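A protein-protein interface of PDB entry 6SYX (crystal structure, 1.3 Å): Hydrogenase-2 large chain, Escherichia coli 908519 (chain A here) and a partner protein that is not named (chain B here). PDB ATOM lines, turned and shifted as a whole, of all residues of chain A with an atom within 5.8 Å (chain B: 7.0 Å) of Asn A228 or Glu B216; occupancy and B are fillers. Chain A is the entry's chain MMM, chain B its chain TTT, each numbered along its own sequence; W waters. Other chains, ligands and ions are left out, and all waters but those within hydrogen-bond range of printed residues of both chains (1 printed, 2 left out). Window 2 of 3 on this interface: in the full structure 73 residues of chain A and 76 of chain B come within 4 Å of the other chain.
The backbone carbonyl oxygen of Ile A227 lies within hydrogen-bond range of the guanidinium group of Arg B215.
The side-chain amide nitrogen of Asn A228 is in hydrogen-bond range of the backbone carbonyl oxygen of Arg B215 (3.1 Å).
NE of Arg B196 lies close to O of Gly B217 (3.5 Å).
The backbone NH of His B214 is in hydrogen-bond range of the side-chain carboxylate of Asp B211 (2.8 Å).
The backbone carbonyl oxygen of Pro A226 sits at hydrogen-bond distance from the backbone NH of Leu A235 (3.0 Å).
OD1 of Asn A228 sits close to N of Asp A230 (3.1 Å).
The backbone NH (N) of Gly A231 sits at hydrogen-bond distance from the side-chain amide oxygen (OD1) of Asn A228, at 3.4 Å.
The backbone NH of Asn A228 is in hydrogen-bond range of the backbone carbonyl oxygen of Leu A235, 3.0 Å away.
Among the printed residues, pairs that only touch across the chains: His A455 with Arg B215 (3.5 Å), Val A234 with Gly B217 (3.5 Å), Asn A228 with Glu B216 (3.5 Å), Pro A226 with His B214 (3.6 Å), Val A234 with Arg B215 (3.7 Å), Val A234 with His B214 (3.7 Å), Leu A232 with Glu B216 (3.8 Å) and Pro A226 with Arg B215 (3.8 Å).
Of the printed residues of chain B, Val A234 touches His B214 (3.7 Å), Arg B215 (3.7 Å) and Gly B217 (3.5 Å).
Of the printed residues of chain A, His B214 touches Pro A226 and Val A234.
Printed residues of chain A within 4 Å of Arg B215: Pro A226 (3.8 Å), Ile A227 (2.8 Å), Asn A228 (3.1 Å), Val A234 (3.7 Å) and His A455 (3.5 Å).
Of the printed residues of chain A, Glu B216 touches Asn A228 and Leu A232.
Of the printed residues of chain A, Gly B217 touches Val A234 (3.5 Å).
The nearest residue of chain B that does not touch Asn A228 is Glu B212 (6.2 Å).
Printed residues of chain B that touch a printed residue of chain A: His B214, Arg B215, Glu B216 and Gly B217.
Hydrophobic or aromatic side chains of chain B within 4 Å of the printed part of chain A: His B214.
Along chain B the printed residues that touch a printed residue of chain A span positions 214 to 217.
Along chain A the printed residues that touch a printed residue of chain B span positions 226 to 455.
Among the printed residues, 10 pairs touch across the chains.
Among the printed residues, no Asp or Glu carboxylate lies within 4 Å of a Lys or Arg side-chain nitrogen of the other chain.
Water W1 bridges OE1 of Glu B216 (2.7 Å) and N of Leu A232 (3.1 Å).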
ATOM      1  N   PRO A 226      20.446   4.905  13.318  1.00  0.00           N
ATOM      2  CA  PRO A 226      21.759   5.178  13.914  1.00  0.00           C
ATOM      3  C   PRO A 226      22.813   5.329  12.813  1.00  0.00           C
ATOM      4  O   PRO A 226      23.134   4.352  12.122  1.00  0.00           O
ATOM      5  CB  PRO A 226      22.037   3.928  14.780  1.00  0.00           C
ATOM      6  CG  PRO A 226      20.930   2.923  14.463  1.00  0.00           C
ATOM      7  CD  PRO A 226      20.214   3.439  13.213  1.00  0.00           C
ATOM      8  N   ILE A 227      23.336   6.544  12.612  1.00  0.00           N
ATOM      9  CA  ILE A 227      24.357   6.807  11.566  1.00  0.00           C
ATOM     10  C   ILE A 227      25.727   6.375  12.074  1.00  0.00           C
ATOM     11  O   ILE A 227      26.226   6.977  13.038  1.00  0.00           O
ATOM     12  CB  ILE A 227      24.350   8.272  11.119  1.00  0.00           C
ATOM     13  CG1 ILE A 227      23.006   8.651  10.470  1.00  0.00           C
ATOM     14  CG2 ILE A 227      25.575   8.582  10.285  1.00  0.00           C
ATOM     15  CD1 ILE A 227      22.865  10.128  10.072  1.00  0.00           C
ATOM     16  N   ASN A 228      26.356   5.422  11.391  1.00  0.00           N
ATOM     17  CA  ASN A 228      27.721   4.976  11.744  1.00  0.00           C
ATOM     18  C   ASN A 228      28.310   4.261  10.522  1.00  0.00           C
ATOM     19  O   ASN A 228      27.978   3.091  10.296  1.00  0.00           O
ATOM     20  CB  ASN A 228      27.750   4.089  12.970  1.00  0.00           C
ATOM     21  CG  ASN A 228      29.149   3.674  13.392  1.00  0.00           C
ATOM     22  OD1 ASN A 228      30.141   4.015  12.724  1.00  0.00           O
ATOM     23  ND2 ASN A 228      29.203   2.908  14.463  1.00  0.00           N
ATOM     24  N   LEU A 229      29.120   4.937   9.707  1.00  0.00           N
ATOM     25  CA  LEU A 229      29.649   4.353   8.457  1.00  0.00           C
ATOM     26  C   LEU A 229      30.425   3.090   8.725  1.00  0.00           C
ATOM     27  O   LEU A 229      30.481   2.236   7.776  1.00  0.00           O
ATOM     28  CB  LEU A 229      30.543   5.331   7.687  1.00  0.00           C
ATOM     29  CG  LEU A 229      29.876   6.619   7.164  1.00  0.00           C
ATOM     30  CD1 LEU A 229      30.816   7.320   6.200  1.00  0.00           C
ATOM     31  CD2 LEU A 229      28.525   6.397   6.484  1.00  0.00           C
ATOM     32  N   ASP A 230      30.995   2.933   9.923  1.00  0.00           N
ATOM     33  CA  ASP A 230      31.859   1.800  10.320  1.00  0.00           C
ATOM     34  C   ASP A 230      31.129   0.766  11.164  1.00  0.00           C
ATOM     35  O   ASP A 230      31.794  -0.171  11.656  1.00  0.00           O
ATOM     36  CB  ASP A 230      33.129   2.362  10.930  1.00  0.00           C
ATOM     37  CG  ASP A 230      33.951   3.141   9.933  1.00  0.00           C
ATOM     38  OD1 ASP A 230      34.355   2.591   8.849  1.00  0.00           O
ATOM     39  OD2 ASP A 230      34.132   4.375  10.189  1.00  0.00           O
ATOM     40  N   GLY A 231      29.796   0.905  11.342  1.00  0.00           N
ATOM     41  CA  GLY A 231      29.044  -0.003  12.212  1.00  0.00           C
ATOM     42  C   GLY A 231      28.357  -1.171  11.514  1.00  0.00           C
ATOM     43  O   GLY A 231      27.803  -0.990  10.434  1.00  0.00           O
ATOM     44  N   LEU A 232      28.363  -2.337  12.108  1.00  0.00           N
ATOM     45  CA  LEU A 232      27.593  -3.535  11.693  1.00  0.00           C
ATOM     46  C   LEU A 232      26.167  -3.379  12.206  1.00  0.00           C
ATOM     47  O   LEU A 232      25.951  -3.027  13.384  1.00  0.00           O
ATOM     48  CB  LEU A 232      28.356  -4.774  12.233  1.00  0.00           C
ATOM     49  CG  LEU A 232      27.824  -6.124  11.757  1.00  0.00           C
ATOM     50  CD1 LEU A 232      28.996  -7.118  11.748  1.00  0.00           C
ATOM     51  CD2 LEU A 232      26.714  -6.630  12.636  1.00  0.00           C
ATOM     52  N   VAL A 234      23.739  -1.199  11.431  1.00  0.00           N
ATOM     53  CA  VAL A 234      23.186   0.181  11.528  1.00  0.00           C
ATOM     54  C   VAL A 234      23.253   0.890  10.166  1.00  0.00           C
ATOM     55  O   VAL A 234      23.542   0.199   9.143  1.00  0.00           O
ATOM     56  CB  VAL A 234      23.928   0.922  12.655  1.00  0.00           C
ATOM     57  CG1 VAL A 234      23.763   0.228  14.023  1.00  0.00           C
ATOM     58  CG2 VAL A 234      25.399   1.119  12.342  1.00  0.00           C
ATOM     59  N   LEU A 235      22.996   2.198  10.099  1.00  0.00           N
ATOM     60  CA  LEU A 235      22.942   2.942   8.820  1.00  0.00           C
ATOM     61  C   LEU A 235      24.404   3.273   8.461  1.00  0.00           C
ATOM     62  O   LEU A 235      24.980   4.301   8.932  1.00  0.00           O
ATOM     63  CB  LEU A 235      22.038   4.184   8.932  1.00  0.00           C
ATOM     64  CG  LEU A 235      21.842   4.993   7.646  1.00  0.00           C
ATOM     65  CD1 LEU A 235      21.256   4.120   6.537  1.00  0.00           C
ATOM     66  CD2 LEU A 235      20.915   6.177   7.903  1.00  0.00           C
ATOM     67  N   ASN A 236      25.004   2.393   7.645  1.00  0.00           N
ATOM     68  CA  ASN A 236      26.437   2.489   7.267  1.00  0.00           C
ATOM     69  C   ASN A 236      26.545   2.819   5.761  1.00  0.00           C
ATOM     70  O   ASN A 236      25.536   3.126   5.111  1.00  0.00           O
ATOM     71  CB  ASN A 236      27.158   1.207   7.699  1.00  0.00           C
ATOM     72  CG  ASN A 236      26.582  -0.037   7.026  1.00  0.00           C
ATOM     73  OD1 ASN A 236      26.091   0.072   5.893  1.00  0.00           O
ATOM     74  ND2 ASN A 236      26.790  -1.210   7.637  1.00  0.00           N
ATOM     75  N   LEU A 237      27.751   2.852   5.191  1.00  0.00           N
ATOM     76  CA  LEU A 237      27.890   3.298   3.779  1.00  0.00           C
ATOM     77  C   LEU A 237      27.257   2.267   2.836  1.00  0.00           C
ATOM     78  O   LEU A 237      26.663   2.673   1.827  1.00  0.00           O
ATOM     79  CB  LEU A 237      29.356   3.576   3.427  1.00  0.00           C
ATOM     80  CG  LEU A 237      29.607   4.207   2.058  1.00  0.00           C
ATOM     81  CD1 LEU A 237      28.856   5.545   1.917  1.00  0.00           C
ATOM     82  CD2 LEU A 237      31.120   4.393   1.840  1.00  0.00           C
ATOM     83  N   HIS A 455      27.377  12.866  12.950  1.00  0.00           N
ATOM     84  CA  HIS A 455      26.542  11.642  12.979  1.00  0.00           C
ATOM     85  C   HIS A 455      25.281  11.844  13.848  1.00  0.00           C
ATOM     86  O   HIS A 455      24.597  10.835  14.154  1.00  0.00           O
ATOM     87  CB  HIS A 455      27.347  10.414  13.413  1.00  0.00           C
ATOM     88  CG  HIS A 455      27.887  10.526  14.806  1.00  0.00           C
ATOM     89  ND1 HIS A 455      29.268  10.707  15.069  1.00  0.00           N
ATOM     90  CD2 HIS A 455      27.274  10.522  16.012  1.00  0.00           C
ATOM     91  CE1 HIS A 455      29.438  10.799  16.381  1.00  0.00           C
ATOM     92  NE2 HIS A 455      28.260  10.732  16.995  1.00  0.00           N
ATOM     93  N   ARG B 196      19.042  -9.650  17.794  1.00  0.00           N
ATOM     94  CA  ARG B 196      19.681  -8.875  18.883  1.00  0.00           C
ATOM     95  C   ARG B 196      19.597  -9.600  20.240  1.00  0.00           C
ATOM     96  O   ARG B 196      20.110  -9.069  21.242  1.00  0.00           O
ATOM     97  CB  ARG B 196      19.077  -7.466  18.950  1.00  0.00           C
ATOM     98  CG  ARG B 196      19.205  -6.720  17.620  1.00  0.00           C
ATOM     99  CD  ARG B 196      19.014  -5.228  17.705  1.00  0.00           C
ATOM    100  NE  ARG B 196      19.257  -4.663  16.373  1.00  0.00           N
ATOM    101  CZ  ARG B 196      19.495  -3.372  16.150  1.00  0.00           C
ATOM    102  NH1 ARG B 196      19.476  -2.478  17.137  1.00  0.00           N
ATOM    103  NH2 ARG B 196      19.798  -2.983  14.923  1.00  0.00           N
ATOM    104  N   HIS B 199      22.707  -9.582  22.547  1.00  0.00           N
ATOM    105  CA  HIS B 199      22.933  -8.285  23.250  1.00  0.00           C
ATOM    106  C   HIS B 199      22.005  -8.210  24.483  1.00  0.00           C
ATOM    107  O   HIS B 199      22.496  -7.856  25.575  1.00  0.00           O
ATOM    108  CB  HIS B 199      22.669  -7.106  22.296  1.00  0.00           C
ATOM    109  CG  HIS B 199      23.523  -7.181  21.066  1.00  0.00           C
ATOM    110  ND1 HIS B 199      24.924  -7.299  21.159  1.00  0.00           N
ATOM    111  CD2 HIS B 199      23.199  -7.239  19.731  1.00  0.00           C
ATOM    112  CE1 HIS B 199      25.403  -7.363  19.923  1.00  0.00           C
ATOM    113  NE2 HIS B 199      24.378  -7.352  19.039  1.00  0.00           N
ATOM    114  N   ASP B 211      22.812   7.086  20.903  1.00  0.00           N
ATOM    115  CA  ASP B 211      23.917   6.821  21.885  1.00  0.00           C
ATOM    116  C   ASP B 211      24.846   5.744  21.326  1.00  0.00           C
ATOM    117  O   ASP B 211      24.653   5.212  20.227  1.00  0.00           O
ATOM    118  CB  ASP B 211      23.431   6.525  23.300  1.00  0.00           C
ATOM    119  CG  ASP B 211      22.864   5.153  23.609  1.00  0.00           C
ATOM    120  OD1 ASP B 211      22.934   4.239  22.700  1.00  0.00           O
ATOM    121  OD2 ASP B 211      22.366   4.947  24.751  1.00  0.00           O
ATOM    122  N   GLU B 212      25.950   5.477  22.040  1.00  0.00           N
ATOM    123  CA  GLU B 212      27.046   4.633  21.464  1.00  0.00           C
ATOM    124  C   GLU B 212      26.528   3.211  21.270  1.00  0.00           C
ATOM    125  O   GLU B 212      26.795   2.658  20.177  1.00  0.00           O
ATOM    126  CB  GLU B 212      28.269   4.714  22.388  1.00  0.00           C
ATOM    127  CG  GLU B 212      29.526   4.012  21.924  1.00  0.00           C
ATOM    128  CD  GLU B 212      30.616   4.287  22.978  1.00  0.00           C
ATOM    129  OE1 GLU B 212      30.830   3.405  23.844  1.00  0.00           O
ATOM    130  OE2 GLU B 212      31.164   5.433  22.992  1.00  0.00           O
ATOM    131  N   GLY B 213      25.756   2.642  22.181  1.00  0.00           N
ATOM    132  CA  GLY B 213      25.208   1.275  22.008  1.00  0.00           C
ATOM    133  C   GLY B 213      24.179   1.198  20.877  1.00  0.00           C
ATOM    134  O   GLY B 213      24.194   0.219  20.081  1.00  0.00           O
ATOM    135  N   HIS B 214      23.307   2.194  20.765  1.00  0.00           N
ATOM    136  CA  HIS B 214      22.343   2.277  19.628  1.00  0.00           C
ATOM    137  C   HIS B 214      23.085   2.267  18.287  1.00  0.00           C
ATOM    138  O   HIS B 214      22.681   1.535  17.349  1.00  0.00           O
ATOM    139  CB  HIS B 214      21.521   3.546  19.770  1.00  0.00           C
ATOM    140  CG  HIS B 214      20.379   3.664  18.800  1.00  0.00           C
ATOM    141  ND1 HIS B 214      20.321   4.729  17.933  1.00  0.00           N
ATOM    142  CD2 HIS B 214      19.348   2.829  18.535  1.00  0.00           C
ATOM    143  CE1 HIS B 214      19.202   4.589  17.226  1.00  0.00           C
ATOM    144  NE2 HIS B 214      18.592   3.451  17.566  1.00  0.00           N
ATOM    145  N   ARG B 215      24.211   3.000  18.192  1.00  0.00           N
ATOM    146  CA  ARG B 215      25.061   3.093  16.993  1.00  0.00           C
ATOM    147  C   ARG B 215      25.936   1.847  16.789  1.00  0.00           C
ATOM    148  O   ARG B 215      26.636   1.812  15.759  1.00  0.00           O
ATOM    149  CB  ARG B 215      25.836   4.422  16.999  1.00  0.00           C
ATOM    150  CG  ARG B 215      24.929   5.634  16.807  1.00  0.00           C
ATOM    151  CD  ARG B 215      25.678   6.990  16.934  1.00  0.00           C
ATOM    152  NE  ARG B 215      26.601   7.135  15.828  1.00  0.00           N
ATOM    153  CZ  ARG B 215      27.929   7.129  15.890  1.00  0.00           C
ATOM    154  NH1 ARG B 215      28.513   7.145  17.094  1.00  0.00           N
ATOM    155  NH2 ARG B 215      28.650   7.120  14.770  1.00  0.00           N
ATOM    156  N   GLU B 216      25.852   0.863  17.679  1.00  0.00           N
ATOM    157  CA  GLU B 216      26.504  -0.463  17.472  1.00  0.00           C
ATOM    158  C   GLU B 216      25.458  -1.553  17.246  1.00  0.00           C
ATOM    159  O   GLU B 216      25.815  -2.739  17.195  1.00  0.00           O
ATOM    160  CB  GLU B 216      27.481  -0.827  18.600  1.00  0.00           C
ATOM    161  CG  GLU B 216      28.657   0.145  18.787  1.00  0.00           C
ATOM    162  CD  GLU B 216      29.592   0.285  17.576  1.00  0.00           C
ATOM    163  OE1 GLU B 216      29.665  -0.664  16.687  1.00  0.00           O
ATOM    164  OE2 GLU B 216      30.276   1.377  17.475  1.00  0.00           O
ATOM    165  N   GLY B 217      24.157  -1.247  17.149  1.00  0.00           N
ATOM    166  CA  GLY B 217      23.135  -2.279  16.861  1.00  0.00           C
ATOM    167  C   GLY B 217      22.773  -3.137  18.069  1.00  0.00           C
ATOM    168  O   GLY B 217      22.317  -4.284  17.924  1.00  0.00           O
ATOM    169  N   TRP B 218      22.832  -2.585  19.296  1.00  0.00           N
ATOM    170  CA  TRP B 218      22.487  -3.318  20.541  1.00  0.00           C
ATOM    171  C   TRP B 218      20.976  -3.472  20.722  1.00  0.00           C
ATOM    172  O   TRP B 218      20.145  -2.911  19.965  1.00  0.00           O
ATOM    173  CB  TRP B 218      23.148  -2.647  21.763  1.00  0.00           C
ATOM    174  CG  TRP B 218      24.638  -2.766  21.838  1.00  0.00           C
ATOM    175  CD1 TRP B 218      25.486  -3.391  20.972  1.00  0.00           C
ATOM    176  CD2 TRP B 218      25.481  -2.241  22.897  1.00  0.00           C
ATOM    177  NE1 TRP B 218      26.798  -3.312  21.430  1.00  0.00           N
ATOM    178  CE2 TRP B 218      26.824  -2.604  22.608  1.00  0.00           C
ATOM    179  CE3 TRP B 218      25.206  -1.522  24.063  1.00  0.00           C
ATOM    180  CZ2 TRP B 218      27.899  -2.249  23.440  1.00  0.00           C
ATOM    181  CZ3 TRP B 218      26.263  -1.191  24.899  1.00  0.00           C
ATOM    182  CH2 TRP B 218      27.576  -1.562  24.597  1.00  0.00           C
HETATM  183  O   HOH W   1      28.439  -2.605  15.181  1.00  0.00           O
